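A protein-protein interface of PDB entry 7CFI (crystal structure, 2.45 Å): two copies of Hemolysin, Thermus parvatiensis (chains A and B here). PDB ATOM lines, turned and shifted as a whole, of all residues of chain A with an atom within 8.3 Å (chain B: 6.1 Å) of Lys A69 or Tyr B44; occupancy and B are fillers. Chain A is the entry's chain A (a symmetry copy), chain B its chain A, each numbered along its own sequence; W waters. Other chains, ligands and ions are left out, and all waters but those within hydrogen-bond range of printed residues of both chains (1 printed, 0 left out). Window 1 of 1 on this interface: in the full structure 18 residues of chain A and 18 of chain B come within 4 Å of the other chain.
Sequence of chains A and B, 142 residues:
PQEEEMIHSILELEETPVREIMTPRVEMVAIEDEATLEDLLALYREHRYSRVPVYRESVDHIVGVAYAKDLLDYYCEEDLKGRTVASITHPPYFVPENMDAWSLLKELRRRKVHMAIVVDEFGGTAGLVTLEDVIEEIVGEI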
ATOM      1  N   LEU A  40       8.168   2.432 -22.442  1.00  0.00           N
ATOM      2  CA  LEU A  40       9.480   2.834 -22.938  1.00  0.00           C
ATOM      3  C   LEU A  40       9.654   2.443 -24.398  1.00  0.00           C
ATOM      4  O   LEU A  40      10.208   3.216 -25.194  1.00  0.00           O
ATOM      5  CB  LEU A  40      10.580   2.213 -22.080  1.00  0.00           C
ATOM      6  CG  LEU A  40      12.004   2.617 -22.461  1.00  0.00           C
ATOM      7  CD1 LEU A  40      12.213   4.095 -22.178  1.00  0.00           C
ATOM      8  CD2 LEU A  40      13.034   1.778 -21.724  1.00  0.00           C
ATOM      9  N   TYR A  44      10.348   5.011 -27.218  1.00  0.00           N
ATOM     10  CA  TYR A  44      11.443   4.869 -28.170  1.00  0.00           C
ATOM     11  C   TYR A  44      10.932   4.934 -29.603  1.00  0.00           C
ATOM     12  O   TYR A  44      11.516   5.615 -30.451  1.00  0.00           O
ATOM     13  CB  TYR A  44      12.204   3.562 -27.954  1.00  0.00           C
ATOM     14  CG  TYR A  44      13.233   3.357 -29.043  1.00  0.00           C
ATOM     15  CD1 TYR A  44      14.436   4.050 -29.020  1.00  0.00           C
ATOM     16  CD2 TYR A  44      12.981   2.515 -30.122  1.00  0.00           C
ATOM     17  CE1 TYR A  44      15.371   3.890 -30.021  1.00  0.00           C
ATOM     18  CE2 TYR A  44      13.910   2.353 -31.130  1.00  0.00           C
ATOM     19  CZ  TYR A  44      15.102   3.041 -31.074  1.00  0.00           C
ATOM     20  OH  TYR A  44      16.033   2.882 -32.073  1.00  0.00           O
ATOM     21  N   TYR A  49      15.381   8.205 -29.375  1.00  0.00           N
ATOM     22  CA  TYR A  49      16.562   8.446 -28.557  1.00  0.00           C
ATOM     23  C   TYR A  49      16.998   7.155 -27.878  1.00  0.00           C
ATOM     24  O   TYR A  49      16.170   6.363 -27.420  1.00  0.00           O
ATOM     25  CB  TYR A  49      16.296   9.536 -27.519  1.00  0.00           C
ATOM     26  CG  TYR A  49      16.224  10.921 -28.125  1.00  0.00           C
ATOM     27  CD1 TYR A  49      17.372  11.553 -28.586  1.00  0.00           C
ATOM     28  CD2 TYR A  49      15.016  11.602 -28.226  1.00  0.00           C
ATOM     29  CE1 TYR A  49      17.321  12.819 -29.143  1.00  0.00           C
ATOM     30  CE2 TYR A  49      14.957  12.870 -28.776  1.00  0.00           C
ATOM     31  CZ  TYR A  49      16.108  13.474 -29.230  1.00  0.00           C
ATOM     32  OH  TYR A  49      16.052  14.736 -29.778  1.00  0.00           O
ATOM     33  N   SER A  50      18.314   6.936 -27.837  1.00  0.00           N
ATOM     34  CA  SER A  50      18.848   5.711 -27.255  1.00  0.00           C
ATOM     35  C   SER A  50      18.875   5.768 -25.734  1.00  0.00           C
ATOM     36  O   SER A  50      18.706   4.733 -25.079  1.00  0.00           O
ATOM     37  CB  SER A  50      20.254   5.445 -27.795  1.00  0.00           C
ATOM     38  OG  SER A  50      20.228   5.204 -29.190  1.00  0.00           O
ATOM     39  N   ARG A  51      19.082   6.953 -25.163  1.00  0.00           N
ATOM     40  CA  ARG A  51      19.171   7.138 -23.722  1.00  0.00           C
ATOM     41  C   ARG A  51      18.102   8.126 -23.283  1.00  0.00           C
ATOM     42  O   ARG A  51      17.995   9.224 -23.840  1.00  0.00           O
ATOM     43  CB  ARG A  51      20.567   7.621 -23.321  1.00  0.00           C
ATOM     44  CG  ARG A  51      21.659   6.569 -23.488  1.00  0.00           C
ATOM     45  CD  ARG A  51      23.018   7.048 -22.981  1.00  0.00           C
ATOM     46  NE  ARG A  51      24.135   6.272 -23.516  1.00  0.00           N
ATOM     47  CZ  ARG A  51      24.458   6.184 -24.805  1.00  0.00           C
ATOM     48  NH1 ARG A  51      23.768   6.843 -25.726  1.00  0.00           N
ATOM     49  NH2 ARG A  51      25.492   5.440 -25.177  1.00  0.00           N
ATOM     50  N   ALA A  66      17.706   5.507 -18.644  1.00  0.00           N
ATOM     51  CA  ALA A  66      17.330   4.210 -19.186  1.00  0.00           C
ATOM     52  C   ALA A  66      17.816   4.098 -20.625  1.00  0.00           C
ATOM     53  O   ALA A  66      17.770   5.072 -21.383  1.00  0.00           O
ATOM     54  CB  ALA A  66      15.815   3.992 -19.128  1.00  0.00           C
ATOM     55  N   TYR A  67      18.282   2.913 -21.001  1.00  0.00           N
ATOM     56  CA  TYR A  67      18.729   2.642 -22.362  1.00  0.00           C
ATOM     57  C   TYR A  67      17.638   1.862 -23.085  1.00  0.00           C
ATOM     58  O   TYR A  67      17.177   0.829 -22.591  1.00  0.00           O
ATOM     59  CB  TYR A  67      20.038   1.853 -22.383  1.00  0.00           C
ATOM     60  CG  TYR A  67      21.166   2.441 -21.562  1.00  0.00           C
ATOM     61  CD1 TYR A  67      21.209   3.796 -21.248  1.00  0.00           C
ATOM     62  CD2 TYR A  67      22.192   1.631 -21.099  1.00  0.00           C
ATOM     63  CE1 TYR A  67      22.245   4.320 -20.493  1.00  0.00           C
ATOM     64  CE2 TYR A  67      23.230   2.145 -20.350  1.00  0.00           C
ATOM     65  CZ  TYR A  67      23.252   3.488 -20.047  1.00  0.00           C
ATOM     66  OH  TYR A  67      24.289   3.997 -19.296  1.00  0.00           O
ATOM     67  N   ALA A  68      17.232   2.358 -24.252  1.00  0.00           N
ATOM     68  CA  ALA A  68      16.250   1.646 -25.062  1.00  0.00           C
ATOM     69  C   ALA A  68      16.745   0.259 -25.449  1.00  0.00           C
ATOM     70  O   ALA A  68      15.948  -0.677 -25.553  1.00  0.00           O
ATOM     71  CB  ALA A  68      15.917   2.457 -26.318  1.00  0.00           C
ATOM     72  N   LYS A  69      18.054   0.108 -25.652  1.00  0.00           N
ATOM     73  CA  LYS A  69      18.611  -1.180 -26.053  1.00  0.00           C
ATOM     74  C   LYS A  69      18.421  -2.245 -24.980  1.00  0.00           C
ATOM     75  O   LYS A  69      18.376  -3.439 -25.299  1.00  0.00           O
ATOM     76  CB  LYS A  69      20.097  -1.027 -26.387  1.00  0.00           C
ATOM     77  N   ASP A  70      18.307  -1.842 -23.709  1.00  0.00           N
ATOM     78  CA  ASP A  70      18.090  -2.816 -22.644  1.00  0.00           C
ATOM     79  C   ASP A  70      16.732  -3.495 -22.745  1.00  0.00           C
ATOM     80  O   ASP A  70      16.525  -4.530 -22.105  1.00  0.00           O
ATOM     81  CB  ASP A  70      18.245  -2.152 -21.275  1.00  0.00           C
ATOM     82  CG  ASP A  70      19.690  -1.845 -20.938  1.00  0.00           C
ATOM     83  OD1 ASP A  70      20.585  -2.349 -21.646  1.00  0.00           O
ATOM     84  OD2 ASP A  70      19.931  -1.107 -19.957  1.00  0.00           O
ATOM     85  N   LEU A  71      15.801  -2.931 -23.522  1.00  0.00           N
ATOM     86  CA  LEU A  71      14.544  -3.622 -23.792  1.00  0.00           C
ATOM     87  C   LEU A  71      14.775  -4.927 -24.539  1.00  0.00           C
ATOM     88  O   LEU A  71      13.983  -5.868 -24.411  1.00  0.00           O
ATOM     89  CB  LEU A  71      13.612  -2.732 -24.609  1.00  0.00           C
ATOM     90  CG  LEU A  71      13.052  -1.460 -23.987  1.00  0.00           C
ATOM     91  CD1 LEU A  71      12.226  -0.726 -25.021  1.00  0.00           C
ATOM     92  CD2 LEU A  71      12.209  -1.797 -22.774  1.00  0.00           C
ATOM     93  N   LEU A  72      15.847  -4.999 -25.328  1.00  0.00           N
ATOM     94  CA  LEU A  72      16.126  -6.180 -26.135  1.00  0.00           C
ATOM     95  C   LEU A  72      16.503  -7.393 -25.301  1.00  0.00           C
ATOM     96  O   LEU A  72      16.522  -8.507 -25.833  1.00  0.00           O
ATOM     97  CB  LEU A  72      17.231  -5.858 -27.139  1.00  0.00           C
ATOM     98  CG  LEU A  72      16.745  -4.889 -28.216  1.00  0.00           C
ATOM     99  CD1 LEU A  72      17.867  -4.470 -29.150  1.00  0.00           C
ATOM    100  CD2 LEU A  72      15.612  -5.535 -28.991  1.00  0.00           C
ATOM    101  N   ASP A  73      16.795  -7.211 -24.015  1.00  0.00           N
ATOM    102  CA  ASP A  73      17.065  -8.334 -23.128  1.00  0.00           C
ATOM    103  C   ASP A  73      15.799  -8.983 -22.589  1.00  0.00           C
ATOM    104  O   ASP A  73      15.894  -9.992 -21.881  1.00  0.00           O
ATOM    105  CB  ASP A  73      17.926  -7.880 -21.946  1.00  0.00           C
ATOM    106  CG  ASP A  73      19.347  -7.556 -22.351  1.00  0.00           C
ATOM    107  OD1 ASP A  73      20.021  -8.437 -22.927  1.00  0.00           O
ATOM    108  OD2 ASP A  73      19.792  -6.418 -22.093  1.00  0.00           O
ATOM    109  N   TYR A  74      14.625  -8.441 -22.898  1.00  0.00           N
ATOM    110  CA  TYR A  74      13.391  -8.832 -22.230  1.00  0.00           C
ATOM    111  C   TYR A  74      12.418  -9.448 -23.218  1.00  0.00           C
ATOM    112  O   TYR A  74      12.251  -8.949 -24.337  1.00  0.00           O
ATOM    113  CB  TYR A  74      12.764  -7.641 -21.510  1.00  0.00           C
ATOM    114  CG  TYR A  74      13.582  -7.256 -20.309  1.00  0.00           C
ATOM    115  CD1 TYR A  74      13.494  -7.983 -19.131  1.00  0.00           C
ATOM    116  CD2 TYR A  74      14.472  -6.194 -20.362  1.00  0.00           C
ATOM    117  CE1 TYR A  74      14.250  -7.650 -18.031  1.00  0.00           C
ATOM    118  CE2 TYR A  74      15.233  -5.853 -19.267  1.00  0.00           C
ATOM    119  CZ  TYR A  74      15.120  -6.584 -18.104  1.00  0.00           C
ATOM    120  OH  TYR A  74      15.878  -6.247 -17.009  1.00  0.00           O
ATOM    121  N   ILE A  88      15.338  -1.114 -14.910  1.00  0.00           N
ATOM    122  CA  ILE A  88      16.447  -1.085 -15.853  1.00  0.00           C
ATOM    123  C   ILE A  88      17.216   0.235 -15.773  1.00  0.00           C
ATOM    124  O   ILE A  88      18.061   0.510 -16.618  1.00  0.00           O
ATOM    125  CB  ILE A  88      15.963  -1.337 -17.293  1.00  0.00           C
ATOM    126  CG1 ILE A  88      15.102  -0.186 -17.800  1.00  0.00           C
ATOM    127  CG2 ILE A  88      15.179  -2.650 -17.362  1.00  0.00           C
ATOM    128  CD1 ILE A  88      14.861  -0.230 -19.296  1.00  0.00           C
ATOM    129  N   ASP B  39      17.667 -14.170 -35.111  1.00  0.00           N
ATOM    130  CA  ASP B  39      19.094 -14.440 -34.962  1.00  0.00           C
ATOM    131  C   ASP B  39      19.883 -13.166 -34.687  1.00  0.00           C
ATOM    132  O   ASP B  39      20.934 -13.220 -34.038  1.00  0.00           O
ATOM    133  CB  ASP B  39      19.640 -15.146 -36.205  1.00  0.00           C
ATOM    134  CG  ASP B  39      18.811 -16.351 -36.601  1.00  0.00           C
ATOM    135  OD1 ASP B  39      18.485 -17.162 -35.707  1.00  0.00           O
ATOM    136  OD2 ASP B  39      18.502 -16.502 -37.801  1.00  0.00           O
ATOM    137  N   LEU B  40      19.407 -12.019 -35.179  1.00  0.00           N
ATOM    138  CA  LEU B  40      20.056 -10.756 -34.843  1.00  0.00           C
ATOM    139  C   LEU B  40      19.836 -10.404 -33.379  1.00  0.00           C
ATOM    140  O   LEU B  40      20.758  -9.922 -32.704  1.00  0.00           O
ATOM    141  CB  LEU B  40      19.537  -9.641 -35.748  1.00  0.00           C
ATOM    142  CG  LEU B  40      20.194  -8.277 -35.537  1.00  0.00           C
ATOM    143  CD1 LEU B  40      21.653  -8.338 -35.956  1.00  0.00           C
ATOM    144  CD2 LEU B  40      19.461  -7.185 -36.298  1.00  0.00           C
ATOM    145  N   LEU B  41      18.615 -10.628 -32.882  1.00  0.00           N
ATOM    146  CA  LEU B  41      18.334 -10.466 -31.460  1.00  0.00           C
ATOM    147  C   LEU B  41      19.257 -11.335 -30.614  1.00  0.00           C
ATOM    148  O   LEU B  41      19.834 -10.874 -29.622  1.00  0.00           O
ATOM    149  CB  LEU B  41      16.871 -10.810 -31.190  1.00  0.00           C
ATOM    150  CG  LEU B  41      16.283 -10.494 -29.820  1.00  0.00           C
ATOM    151  CD1 LEU B  41      16.091  -9.005 -29.635  1.00  0.00           C
ATOM    152  CD2 LEU B  41      14.959 -11.223 -29.665  1.00  0.00           C
ATOM    153  N   ALA B  42      19.400 -12.605 -30.993  1.00  0.00           N
ATOM    154  CA  ALA B  42      20.308 -13.499 -30.283  1.00  0.00           C
ATOM    155  C   ALA B  42      21.744 -13.003 -30.376  1.00  0.00           C
ATOM    156  O   ALA B  42      22.475 -12.988 -29.380  1.00  0.00           O
ATOM    157  CB  ALA B  42      20.191 -14.916 -30.845  1.00  0.00           C
ATOM    158  N   LEU B  43      22.166 -12.588 -31.572  1.00  0.00           N
ATOM    159  CA  LEU B  43      23.514 -12.057 -31.741  1.00  0.00           C
ATOM    160  C   LEU B  43      23.725 -10.818 -30.883  1.00  0.00           C
ATOM    161  O   LEU B  43      24.773 -10.664 -30.245  1.00  0.00           O
ATOM    162  CB  LEU B  43      23.778 -11.743 -33.215  1.00  0.00           C
ATOM    163  CG  LEU B  43      25.205 -11.313 -33.557  1.00  0.00           C
ATOM    164  CD1 LEU B  43      26.142 -12.513 -33.608  1.00  0.00           C
ATOM    165  CD2 LEU B  43      25.238 -10.538 -34.865  1.00  0.00           C
ATOM    166  N   TYR B  44      22.736  -9.919 -30.852  1.00  0.00           N
ATOM    167  CA  TYR B  44      22.858  -8.743 -29.999  1.00  0.00           C
ATOM    168  C   TYR B  44      22.976  -9.141 -28.534  1.00  0.00           C
ATOM    169  O   TYR B  44      23.818  -8.611 -27.802  1.00  0.00           O
ATOM    170  CB  TYR B  44      21.672  -7.796 -30.181  1.00  0.00           C
ATOM    171  CG  TYR B  44      21.735  -6.664 -29.180  1.00  0.00           C
ATOM    172  CD1 TYR B  44      22.603  -5.597 -29.372  1.00  0.00           C
ATOM    173  CD2 TYR B  44      20.970  -6.686 -28.019  1.00  0.00           C
ATOM    174  CE1 TYR B  44      22.687  -4.571 -28.454  1.00  0.00           C
ATOM    175  CE2 TYR B  44      21.051  -5.665 -27.093  1.00  0.00           C
ATOM    176  CZ  TYR B  44      21.909  -4.611 -27.316  1.00  0.00           C
ATOM    177  OH  TYR B  44      21.993  -3.590 -26.400  1.00  0.00           O
ATOM    178  N   ARG B  45      22.128 -10.070 -28.090  1.00  0.00           N
ATOM    179  CA  ARG B  45      22.123 -10.463 -26.685  1.00  0.00           C
ATOM    180  C   ARG B  45      23.467 -11.030 -26.249  1.00  0.00           C
ATOM    181  O   ARG B  45      23.834 -10.924 -25.073  1.00  0.00           O
ATOM    182  CB  ARG B  45      21.004 -11.475 -26.433  1.00  0.00           C
ATOM    183  CG  ARG B  45      19.646 -10.837 -26.185  1.00  0.00           C
ATOM    184  CD  ARG B  45      18.594 -11.878 -25.835  1.00  0.00           C
ATOM    185  NE  ARG B  45      17.236 -11.358 -25.986  1.00  0.00           N
ATOM    186  CZ  ARG B  45      16.180 -12.099 -26.306  1.00  0.00           C
ATOM    187  NH1 ARG B  45      16.319 -13.401 -26.520  1.00  0.00           N
ATOM    188  NH2 ARG B  45      14.986 -11.537 -26.411  1.00  0.00           N
ATOM    189  N   GLU B  46      24.222 -11.612 -27.182  1.00  0.00           N
ATOM    190  CA  GLU B  46      25.493 -12.230 -26.827  1.00  0.00           C
ATOM    191  C   GLU B  46      26.639 -11.222 -26.823  1.00  0.00           C
ATOM    192  O   GLU B  46      27.504 -11.272 -25.939  1.00  0.00           O
ATOM    193  CB  GLU B  46      25.797 -13.380 -27.788  1.00  0.00           C
ATOM    194  N   HIS B  47      26.661 -10.296 -27.789  1.00  0.00           N
ATOM    195  CA  HIS B  47      27.827  -9.450 -28.008  1.00  0.00           C
ATOM    196  C   HIS B  47      27.613  -7.966 -27.731  1.00  0.00           C
ATOM    197  O   HIS B  47      28.603  -7.255 -27.523  1.00  0.00           O
ATOM    198  CB  HIS B  47      28.339  -9.618 -29.447  1.00  0.00           C
ATOM    199  CG  HIS B  47      28.866 -10.990 -29.737  1.00  0.00           C
ATOM    200  ND1 HIS B  47      28.067 -12.018 -30.191  1.00  0.00           N
ATOM    201  CD2 HIS B  47      30.109 -11.510 -29.610  1.00  0.00           C
ATOM    202  CE1 HIS B  47      28.798 -13.107 -30.346  1.00  0.00           C
ATOM    203  NE2 HIS B  47      30.041 -12.826 -29.999  1.00  0.00           N
ATOM    204  N   ARG B  48      26.370  -7.481 -27.738  1.00  0.00           N
ATOM    205  CA  ARG B  48      25.983  -6.138 -27.299  1.00  0.00           C
ATOM    206  C   ARG B  48      26.470  -5.020 -28.212  1.00  0.00           C
ATOM    207  O   ARG B  48      26.469  -3.853 -27.798  1.00  0.00           O
ATOM    208  CB  ARG B  48      26.451  -5.846 -25.867  1.00  0.00           C
ATOM    209  CG  ARG B  48      25.946  -6.848 -24.845  1.00  0.00           C
ATOM    210  CD  ARG B  48      24.509  -7.230 -25.155  1.00  0.00           C
ATOM    211  NE  ARG B  48      23.872  -7.987 -24.084  1.00  0.00           N
ATOM    212  CZ  ARG B  48      23.184  -7.430 -23.094  1.00  0.00           C
ATOM    213  NH1 ARG B  48      23.049  -6.112 -23.043  1.00  0.00           N
ATOM    214  NH2 ARG B  48      22.631  -8.189 -22.158  1.00  0.00           N
ATOM    215  N   TYR B  49      26.870  -5.325 -29.441  1.00  0.00           N
ATOM    216  CA  TYR B  49      27.215  -4.269 -30.384  1.00  0.00           C
ATOM    217  C   TYR B  49      25.951  -3.681 -30.995  1.00  0.00           C
ATOM    218  O   TYR B  49      24.999  -4.401 -31.309  1.00  0.00           O
ATOM    219  CB  TYR B  49      28.147  -4.793 -31.476  1.00  0.00           C
ATOM    220  CG  TYR B  49      29.554  -5.043 -30.979  1.00  0.00           C
ATOM    221  CD1 TYR B  49      30.400  -3.982 -30.681  1.00  0.00           C
ATOM    222  CD2 TYR B  49      30.043  -6.335 -30.819  1.00  0.00           C
ATOM    223  CE1 TYR B  49      31.689  -4.196 -30.225  1.00  0.00           C
ATOM    224  CE2 TYR B  49      31.332  -6.558 -30.369  1.00  0.00           C
ATOM    225  CZ  TYR B  49      32.150  -5.490 -30.077  1.00  0.00           C
ATOM    226  OH  TYR B  49      33.434  -5.709 -29.628  1.00  0.00           O
ATOM    227  N   SER B  50      25.938  -2.355 -31.142  1.00  0.00           N
ATOM    228  CA  SER B  50      24.763  -1.675 -31.672  1.00  0.00           C
ATOM    229  C   SER B  50      24.679  -1.779 -33.189  1.00  0.00           C
ATOM    230  O   SER B  50      23.574  -1.828 -33.740  1.00  0.00           O
ATOM    231  CB  SER B  50      24.773  -0.206 -31.248  1.00  0.00           C
ATOM    232  OG  SER B  50      24.664  -0.080 -29.841  1.00  0.00           O
ATOM    233  N   ALA B  68      20.929  -2.951 -34.232  1.00  0.00           N
ATOM    234  CA  ALA B  68      20.152  -3.735 -33.278  1.00  0.00           C
ATOM    235  C   ALA B  68      18.902  -2.989 -32.830  1.00  0.00           C
ATOM    236  O   ALA B  68      17.867  -3.609 -32.576  1.00  0.00           O
ATOM    237  CB  ALA B  68      21.015  -4.095 -32.066  1.00  0.00           C
ATOM    238  N   LEU B  71      15.436  -3.545 -34.397  1.00  0.00           N
ATOM    239  CA  LEU B  71      14.585  -4.645 -33.956  1.00  0.00           C
ATOM    240  C   LEU B  71      13.409  -4.143 -33.132  1.00  0.00           C
ATOM    241  O   LEU B  71      12.348  -4.777 -33.108  1.00  0.00           O
ATOM    242  CB  LEU B  71      15.390  -5.643 -33.128  1.00  0.00           C
ATOM    243  CG  LEU B  71      16.494  -6.452 -33.795  1.00  0.00           C
ATOM    244  CD1 LEU B  71      17.184  -7.303 -32.749  1.00  0.00           C
ATOM    245  CD2 LEU B  71      15.916  -7.322 -34.892  1.00  0.00           C
ATOM    246  N   LEU B  72      13.581  -3.014 -32.444  1.00  0.00           N
ATOM    247  CA  LEU B  72      12.540  -2.481 -31.575  1.00  0.00           C
ATOM    248  C   LEU B  72      11.328  -1.977 -32.341  1.00  0.00           C
ATOM    249  O   LEU B  72      10.286  -1.732 -31.726  1.00  0.00           O
ATOM    250  CB  LEU B  72      13.125  -1.367 -30.709  1.00  0.00           C
ATOM    251  CG  LEU B  72      14.103  -1.918 -29.671  1.00  0.00           C
ATOM    252  CD1 LEU B  72      14.779  -0.810 -28.884  1.00  0.00           C
ATOM    253  CD2 LEU B  72      13.363  -2.864 -28.744  1.00  0.00           C
HETATM  254  O   HOH W   1      12.182  -9.777 -26.679  1.00  0.00           O
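The backbone carbonyl oxygen (O) of Leu A72 sits at hydrogen-bond distance from the guanidinium group (NE) of Arg B45, 2.9 Å away.
The side-chain carboxylate (OD1) of Asp A73 is in salt-bridge range of the guanidinium group (NH2) of Arg B48.
O of Arg B45 sits at hydrogen-bond distance from NE of Arg B48 (3.1 Å).
The backbone carbonyl oxygen of Ser B50 sits at hydrogen-bond distance from the backbone NH of Ala B68.
N of Ala A68 sits at hydrogen-bond distance from O of Ser A50, 2.9 Å away.
Leu B72 touches Tyr A44 (CB to CE2, 3.8 Å).
Ala A68 touches Leu B72 (O to CD1, 3.5 Å).
Tyr B44 touches Lys A69.
CD2 of Leu A72 touches CD1 of Leu B41, 3.6 Å away.
CB of Leu A72 touches CE2 of Tyr B44, 3.8 Å away.
Leu A72 touches Ala B68 (CD1 to O, 3.5 Å).
Leu B72 touches Leu A72 (CD2 to CD2, 3.5 Å).
Tyr B44 touches two residues of chain A.
Of the printed residues of chain B, Ala A68 touches Leu B72.
Printed residues of chain A within 4 Å of Arg B48: Asp A73 (2.7 Å).
Tyr A49 touches none of the printed residues of chain B.
Ala A66 touches none of the printed residues of chain B.
The nearest residue of chain B that does not touch Lys A69 is Leu B72 (4.7 Å).
The nearest residue of chain A that does not touch Tyr B44 is Asp A70 (4.9 Å).
Of the 15 printed residues of chain B, 6 touch a printed residue of chain A.
Printed residues of chain B that touch a printed residue of chain A: Leu B41, Tyr B44, Arg B45, Arg B48, Ala B68 and Leu B72.
Tyr A44 touches Leu B72, and with the chains exchanged Leu A72 touches Tyr B44.
Ala A68 touches Leu B72, and with the chains exchanged Leu A72 touches Ala B68.
Leu B72 touches its own counterpart, Leu A72.
Positions printed for both chains: 40, 44, 49, 50, 68, 71 and 72.
Water W1 lies within hydrogen-bond range of O of Tyr A74 (2.5 Å) and NH2 of Arg B45 (3.3 Å).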
